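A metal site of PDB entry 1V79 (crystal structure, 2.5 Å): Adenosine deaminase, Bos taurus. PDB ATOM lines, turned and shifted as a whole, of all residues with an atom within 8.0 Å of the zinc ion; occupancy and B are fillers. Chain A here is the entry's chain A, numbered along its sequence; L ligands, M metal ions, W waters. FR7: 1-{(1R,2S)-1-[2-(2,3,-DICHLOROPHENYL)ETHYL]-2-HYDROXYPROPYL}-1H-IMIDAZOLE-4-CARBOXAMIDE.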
ATOM      1  N   HIS A  14      25.175   1.134  -1.990  1.00  0.00           N
ATOM      2  CA  HIS A  14      24.178   0.296  -2.639  1.00  0.00           C
ATOM      3  C   HIS A  14      22.695   0.642  -2.303  1.00  0.00           C
ATOM      4  O   HIS A  14      22.116   0.227  -1.298  1.00  0.00           O
ATOM      5  CB  HIS A  14      24.488  -1.223  -2.404  1.00  0.00           C
ATOM      6  CG  HIS A  14      23.523  -2.153  -3.144  1.00  0.00           C
ATOM      7  ND1 HIS A  14      23.926  -3.063  -4.044  1.00  0.00           N
ATOM      8  CD2 HIS A  14      22.142  -2.250  -3.164  1.00  0.00           C
ATOM      9  CE1 HIS A  14      22.859  -3.666  -4.597  1.00  0.00           C
ATOM     10  NE2 HIS A  14      21.702  -3.165  -4.093  1.00  0.00           N
ATOM     11  N   VAL A  15      22.107   1.325  -3.244  1.00  0.00           N
ATOM     12  CA  VAL A  15      20.853   1.965  -3.039  1.00  0.00           C
ATOM     13  C   VAL A  15      20.154   2.428  -4.360  1.00  0.00           C
ATOM     14  O   VAL A  15      20.782   2.975  -5.254  1.00  0.00           O
ATOM     15  CB  VAL A  15      21.014   3.140  -1.974  1.00  0.00           C
ATOM     16  CG1 VAL A  15      21.981   4.257  -2.311  1.00  0.00           C
ATOM     17  CG2 VAL A  15      19.593   3.617  -1.657  1.00  0.00           C
ATOM     18  N   HIS A  16      18.858   2.082  -4.545  1.00  0.00           N
ATOM     19  CA  HIS A  16      18.296   2.420  -5.867  1.00  0.00           C
ATOM     20  C   HIS A  16      17.492   3.706  -5.880  1.00  0.00           C
ATOM     21  O   HIS A  16      16.533   3.895  -5.155  1.00  0.00           O
ATOM     22  CB  HIS A  16      17.397   1.287  -6.420  1.00  0.00           C
ATOM     23  CG  HIS A  16      18.048  -0.070  -6.594  1.00  0.00           C
ATOM     24  ND1 HIS A  16      18.278  -0.612  -7.791  1.00  0.00           N
ATOM     25  CD2 HIS A  16      18.528  -0.932  -5.640  1.00  0.00           C
ATOM     26  CE1 HIS A  16      18.919  -1.801  -7.569  1.00  0.00           C
ATOM     27  NE2 HIS A  16      19.094  -2.024  -6.254  1.00  0.00           N
ATOM     28  N   ARG A 100      22.250   4.340  -7.601  1.00  0.00           N
ATOM     29  CA  ARG A 100      22.147   3.439  -8.800  1.00  0.00           C
ATOM     30  C   ARG A 100      20.789   3.415  -9.363  1.00  0.00           C
ATOM     31  O   ARG A 100      19.758   3.474  -8.686  1.00  0.00           O
ATOM     32  CB  ARG A 100      22.699   1.987  -8.697  1.00  0.00           C
ATOM     33  CG  ARG A 100      22.010   1.057  -7.773  1.00  0.00           C
ATOM     34  CD  ARG A 100      22.700  -0.308  -7.495  1.00  0.00           C
ATOM     35  NE  ARG A 100      24.012  -0.246  -6.881  1.00  0.00           N
ATOM     36  CZ  ARG A 100      24.900  -1.253  -6.774  1.00  0.00           C
ATOM     37  NH1 ARG A 100      24.751  -2.451  -7.298  1.00  0.00           N
ATOM     38  NH2 ARG A 100      25.992  -1.042  -6.108  1.00  0.00           N
ATOM     39  N   CYS A 152      22.671   0.888 -14.024  1.00  0.00           N
ATOM     40  CA  CYS A 152      22.300  -0.508 -14.191  1.00  0.00           C
ATOM     41  C   CYS A 152      21.788  -1.006 -15.558  1.00  0.00           C
ATOM     42  O   CYS A 152      20.770  -0.694 -16.039  1.00  0.00           O
ATOM     43  CB  CYS A 152      21.162  -0.860 -13.284  1.00  0.00           C
ATOM     44  SG  CYS A 152      21.343  -0.138 -11.711  1.00  0.00           S
ATOM     45  N   ASP A 180      26.377  -1.449 -13.438  1.00  0.00           N
ATOM     46  CA  ASP A 180      25.820  -2.514 -12.658  1.00  0.00           C
ATOM     47  C   ASP A 180      24.958  -3.466 -13.464  1.00  0.00           C
ATOM     48  O   ASP A 180      24.444  -3.155 -14.555  1.00  0.00           O
ATOM     49  CB  ASP A 180      24.951  -1.984 -11.541  1.00  0.00           C
ATOM     50  CG  ASP A 180      24.428  -2.943 -10.477  1.00  0.00           C
ATOM     51  OD1 ASP A 180      23.362  -2.618  -9.971  1.00  0.00           O
ATOM     52  OD2 ASP A 180      25.076  -3.935 -10.112  1.00  0.00           O
ATOM     53  N   LEU A 181      24.773  -4.632 -12.749  1.00  0.00           N
ATOM     54  CA  LEU A 181      23.866  -5.617 -13.207  1.00  0.00           C
ATOM     55  C   LEU A 181      22.757  -5.870 -12.226  1.00  0.00           C
ATOM     56  O   LEU A 181      22.888  -6.391 -11.127  1.00  0.00           O
ATOM     57  CB  LEU A 181      24.659  -6.826 -13.542  1.00  0.00           C
ATOM     58  CG  LEU A 181      23.887  -8.052 -14.111  1.00  0.00           C
ATOM     59  CD1 LEU A 181      22.915  -7.604 -15.185  1.00  0.00           C
ATOM     60  CD2 LEU A 181      24.871  -9.037 -14.704  1.00  0.00           C
ATOM     61  N   ALA A 182      21.652  -5.455 -12.705  1.00  0.00           N
ATOM     62  CA  ALA A 182      20.518  -5.754 -11.862  1.00  0.00           C
ATOM     63  C   ALA A 182      19.332  -6.376 -12.509  1.00  0.00           C
ATOM     64  O   ALA A 182      19.321  -6.455 -13.719  1.00  0.00           O
ATOM     65  CB  ALA A 182      20.067  -4.507 -11.137  1.00  0.00           C
ATOM     66  N   GLY A 183      18.373  -6.782 -11.733  1.00  0.00           N
ATOM     67  CA  GLY A 183      17.138  -7.488 -12.093  1.00  0.00           C
ATOM     68  C   GLY A 183      17.012  -8.883 -11.608  1.00  0.00           C
ATOM     69  O   GLY A 183      17.492  -9.402 -10.696  1.00  0.00           O
ATOM     70  N   HIS A 213      24.754  -7.144  -9.118  1.00  0.00           N
ATOM     71  CA  HIS A 213      23.958  -7.980  -8.147  1.00  0.00           C
ATOM     72  C   HIS A 213      24.093  -9.528  -8.301  1.00  0.00           C
ATOM     73  O   HIS A 213      23.874 -10.125  -9.323  1.00  0.00           O
ATOM     74  CB  HIS A 213      22.484  -7.645  -8.165  1.00  0.00           C
ATOM     75  CG  HIS A 213      22.129  -6.228  -7.883  1.00  0.00           C
ATOM     76  ND1 HIS A 213      22.421  -5.161  -8.637  1.00  0.00           N
ATOM     77  CD2 HIS A 213      21.338  -5.802  -6.813  1.00  0.00           C
ATOM     78  CE1 HIS A 213      21.813  -4.163  -8.034  1.00  0.00           C
ATOM     79  NE2 HIS A 213      21.149  -4.520  -6.913  1.00  0.00           N
ATOM     80  N   GLU A 216      22.253 -12.860  -4.043  1.00  0.00           N
ATOM     81  CA  GLU A 216      21.263 -12.435  -3.043  1.00  0.00           C
ATOM     82  C   GLU A 216      20.151 -13.488  -2.970  1.00  0.00           C
ATOM     83  O   GLU A 216      19.492 -13.698  -1.964  1.00  0.00           O
ATOM     84  CB  GLU A 216      20.700 -11.036  -3.463  1.00  0.00           C
ATOM     85  CG  GLU A 216      19.252 -10.705  -2.944  1.00  0.00           C
ATOM     86  CD  GLU A 216      18.645  -9.418  -3.465  1.00  0.00           C
ATOM     87  OE1 GLU A 216      18.821  -9.116  -4.671  1.00  0.00           O
ATOM     88  OE2 GLU A 216      17.975  -8.712  -2.701  1.00  0.00           O
ATOM     89  N   GLY A 236      27.129  -6.590  -5.408  1.00  0.00           N
ATOM     90  CA  GLY A 236      25.922  -6.452  -4.599  1.00  0.00           C
ATOM     91  C   GLY A 236      25.172  -7.719  -4.095  1.00  0.00           C
ATOM     92  O   GLY A 236      24.844  -8.630  -4.786  1.00  0.00           O
ATOM     93  N   HIS A 237      24.944  -7.686  -2.786  1.00  0.00           N
ATOM     94  CA  HIS A 237      24.733  -8.812  -1.871  1.00  0.00           C
ATOM     95  C   HIS A 237      25.848  -9.872  -1.671  1.00  0.00           C
ATOM     96  O   HIS A 237      26.679  -9.766  -0.821  1.00  0.00           O
ATOM     97  CB  HIS A 237      23.351  -9.307  -2.100  1.00  0.00           C
ATOM     98  CG  HIS A 237      22.348  -8.148  -2.160  1.00  0.00           C
ATOM     99  ND1 HIS A 237      21.733  -7.615  -1.084  1.00  0.00           N
ATOM    100  CD2 HIS A 237      21.710  -7.593  -3.279  1.00  0.00           C
ATOM    101  CE1 HIS A 237      20.730  -6.786  -1.501  1.00  0.00           C
ATOM    102  NE2 HIS A 237      20.727  -6.762  -2.853  1.00  0.00           N
ATOM    103  N   GLU A 259      28.538  -5.580  -0.951  1.00  0.00           N
ATOM    104  CA  GLU A 259      27.474  -4.624  -0.754  1.00  0.00           C
ATOM    105  C   GLU A 259      26.260  -5.089  -0.024  1.00  0.00           C
ATOM    106  O   GLU A 259      25.328  -5.618  -0.641  1.00  0.00           O
ATOM    107  CB  GLU A 259      27.068  -4.030  -2.066  1.00  0.00           C
ATOM    108  CG  GLU A 259      28.210  -3.411  -2.906  1.00  0.00           C
ATOM    109  CD  GLU A 259      27.734  -2.984  -4.264  1.00  0.00           C
ATOM    110  OE1 GLU A 259      26.589  -3.177  -4.633  1.00  0.00           O
ATOM    111  OE2 GLU A 259      28.524  -2.423  -4.970  1.00  0.00           O
ATOM    112  N   CYS A 261      23.026  -5.654   2.162  1.00  0.00           N
ATOM    113  CA  CYS A 261      21.790  -4.948   2.528  1.00  0.00           C
ATOM    114  C   CYS A 261      20.887  -5.625   3.618  1.00  0.00           C
ATOM    115  O   CYS A 261      19.887  -6.247   3.332  1.00  0.00           O
ATOM    116  CB  CYS A 261      20.993  -4.572   1.233  1.00  0.00           C
ATOM    117  SG  CYS A 261      21.955  -4.082  -0.295  1.00  0.00           S
ATOM    118  N   SER A 264      16.620  -5.096   3.885  1.00  0.00           N
ATOM    119  CA  SER A 264      16.370  -5.682   2.550  1.00  0.00           C
ATOM    120  C   SER A 264      16.320  -7.155   2.389  1.00  0.00           C
ATOM    121  O   SER A 264      15.391  -7.728   1.863  1.00  0.00           O
ATOM    122  CB  SER A 264      17.452  -5.384   1.600  1.00  0.00           C
ATOM    123  OG  SER A 264      16.937  -5.532   0.358  1.00  0.00           O
ATOM    124  N   ASN A 292      23.960  -1.167   3.807  1.00  0.00           N
ATOM    125  CA  ASN A 292      23.343  -0.398   2.769  1.00  0.00           C
ATOM    126  C   ASN A 292      21.832  -0.611   2.765  1.00  0.00           C
ATOM    127  O   ASN A 292      21.259  -1.527   3.294  1.00  0.00           O
ATOM    128  CB  ASN A 292      23.717  -0.985   1.428  1.00  0.00           C
ATOM    129  CG  ASN A 292      25.161  -0.782   1.114  1.00  0.00           C
ATOM    130  OD1 ASN A 292      25.485   0.220   0.503  1.00  0.00           O
ATOM    131  ND2 ASN A 292      26.012  -1.720   1.463  1.00  0.00           N
ATOM    132  N   THR A 293      21.222   0.282   2.107  1.00  0.00           N
ATOM    133  CA  THR A 293      19.764   0.276   2.371  1.00  0.00           C
ATOM    134  C   THR A 293      18.816  -0.257   1.373  1.00  0.00           C
ATOM    135  O   THR A 293      17.683  -0.444   1.619  1.00  0.00           O
ATOM    136  CB  THR A 293      19.436   1.706   2.609  1.00  0.00           C
ATOM    137  OG1 THR A 293      19.115   1.922   3.966  1.00  0.00           O
ATOM    138  CG2 THR A 293      18.661   2.414   1.542  1.00  0.00           C
ATOM    139  N   ASP A 294      19.376  -0.371   0.124  1.00  0.00           N
ATOM    140  CA  ASP A 294      18.767  -0.899  -1.069  1.00  0.00           C
ATOM    141  C   ASP A 294      17.631  -0.014  -1.652  1.00  0.00           C
ATOM    142  O   ASP A 294      17.688   0.544  -2.764  1.00  0.00           O
ATOM    143  CB  ASP A 294      18.456  -2.422  -0.877  1.00  0.00           C
ATOM    144  CG  ASP A 294      18.734  -3.296  -2.106  1.00  0.00           C
ATOM    145  OD1 ASP A 294      18.706  -4.554  -2.105  1.00  0.00           O
ATOM    146  OD2 ASP A 294      18.969  -2.671  -3.108  1.00  0.00           O
ATOM    147  N   ASP A 295      16.613   0.064  -0.839  1.00  0.00           N
ATOM    148  CA  ASP A 295      15.394   0.689  -1.285  1.00  0.00           C
ATOM    149  C   ASP A 295      14.588   1.158  -0.074  1.00  0.00           C
ATOM    150  O   ASP A 295      13.669   0.486   0.363  1.00  0.00           O
ATOM    151  CB  ASP A 295      14.457  -0.224  -2.196  1.00  0.00           C
ATOM    152  CG  ASP A 295      14.995  -0.956  -3.449  1.00  0.00           C
ATOM    153  OD1 ASP A 295      14.771  -0.534  -4.598  1.00  0.00           O
ATOM    154  OD2 ASP A 295      15.614  -1.983  -3.283  1.00  0.00           O
ATOM    155  N   PHE A 299      11.150  -1.026   1.226  1.00  0.00           N
ATOM    156  CA  PHE A 299      11.454  -1.567   2.573  1.00  0.00           C
ATOM    157  C   PHE A 299      11.041  -0.764   3.821  1.00  0.00           C
ATOM    158  O   PHE A 299      11.292  -1.236   4.926  1.00  0.00           O
ATOM    159  CB  PHE A 299      12.914  -1.984   2.618  1.00  0.00           C
ATOM    160  CG  PHE A 299      13.257  -2.896   1.449  1.00  0.00           C
ATOM    161  CD1 PHE A 299      12.281  -3.830   0.928  1.00  0.00           C
ATOM    162  CD2 PHE A 299      14.540  -2.798   0.897  1.00  0.00           C
ATOM    163  CE1 PHE A 299      12.601  -4.645  -0.194  1.00  0.00           C
ATOM    164  CE2 PHE A 299      14.863  -3.559  -0.231  1.00  0.00           C
ATOM    165  CZ  PHE A 299      13.908  -4.463  -0.750  1.00  0.00           C
HETATM  166  C1  FR7 L   1      15.944  -2.734  -8.676  1.00  0.00           C
HETATM  167  N2  FR7 L   1      15.665  -1.332  -9.041  1.00  0.00           N
HETATM  168  C3  FR7 L   1      15.154  -0.827  -7.941  1.00  0.00           C
HETATM  169  N4  FR7 L   1      15.163  -1.642  -6.891  1.00  0.00           N
HETATM  170  C5  FR7 L   1      15.699  -2.900  -7.371  1.00  0.00           C
HETATM  171  C8  FR7 L   1      15.959  -4.166  -6.581  1.00  0.00           C
HETATM  172  O9  FR7 L   1      16.062  -5.102  -7.269  1.00  0.00           O
HETATM  173  N10 FR7 L   1      16.033  -4.215  -5.267  1.00  0.00           N
HETATM  174  C13 FR7 L   1      15.501  -0.860 -10.416  1.00  0.00           C
HETATM  175  C14 FR7 L   1      16.911  -0.419 -10.997  1.00  0.00           C
HETATM  176  O15 FR7 L   1      17.793   0.541 -10.352  1.00  0.00           O
HETATM  177  C18 FR7 L   1      14.794  -1.922 -11.333  1.00  0.00           C
HETATM  178  C2  FR7 L   1      13.476  -2.630 -10.824  1.00  0.00           C
HETATM  179  C22 FR7 L   1      12.953  -3.611 -11.810  1.00  0.00           C
HETATM  180  C25 FR7 L   1      12.106  -3.191 -12.828  1.00  0.00           C
HETATM  181  C26 FR7 L   1      11.783  -4.007 -13.930  1.00  0.00           C
HETATM  182  C27 FR7 L   1      12.272  -5.327 -13.997  1.00  0.00           C
HETATM  183  C28 FR7 L   1      12.982  -5.780 -12.904  1.00  0.00           C
HETATM  184  C29 FR7 L   1      13.318  -4.938 -11.835  1.00  0.00           C
HETATM  185 CL1  FR7 L   1      13.385  -7.477 -12.864  1.00  0.00          CL
HETATM  186 CL2  FR7 L   1      14.162  -5.580 -10.500  1.00  0.00          CL
HETATM  187  C9  FR7 L   1      17.943  -1.563 -11.165  1.00  0.00           C
HETATM  188 ZN    ZN M   1      19.951  -3.474  -5.149  1.00  0.00          ZN
HETATM  189  O   HOH W   1      19.341  -5.012  -4.265  1.00  0.00           O
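The side-chain carboxylate of Asp 295 is in hydrogen-bond range of a nitrogen (N4) of the ligand (2.6 Å).
An oxygen (O15) of the ligand is in hydrogen-bond range of a ring nitrogen (ND1) of His 16 (2.9 Å).
The side-chain hydroxyl of Ser 264 lies within hydrogen-bond range of the side-chain carboxylate of Asp 294, 3.2 Å away.
OD1 of Asp 294 sits close to NE2 of His 237 (3.1 Å).
A ring nitrogen (ND1) of His 213 lies within hydrogen-bond range of the backbone carbonyl oxygen (O) of Leu 181.
ND1 of His 14 is in hydrogen-bond range of OE1 of Glu 259 (2.7 Å).
The side-chain amide oxygen (OD1) of Asn 292 lies within hydrogen-bond range of the backbone NH (N) of His 14 (2.7 Å).
ND1 of His 213 lies close to OD1 of Asp 180, at 3.0 Å.
A ring nitrogen (ND1) of His 14 lies within hydrogen-bond range of the guanidinium group (NH1) of Arg 100 (3.4 Å).
The side-chain sulfur (SG) of Cys 261 lies within hydrogen-bond range of the side-chain carboxylate (OD1) of Asp 294.
Of the 21 residues printed, 4 come within 4 Å of the zinc ion.
The nearest printed residue that does not touch the zinc ion is His 237 (4.1 Å).
Water W1 binds the zinc ion (1.9 Å).
The zinc ion is bound by NE2 of His 16.
NE2 of His 14 binds the zinc ion (2.1 Å).
NE2 of His 213 binds the zinc ion.
OD2 of Asp 294 binds the zinc ion, at 2.4 Å.
The zinc ion has five donor atoms within binding distance.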
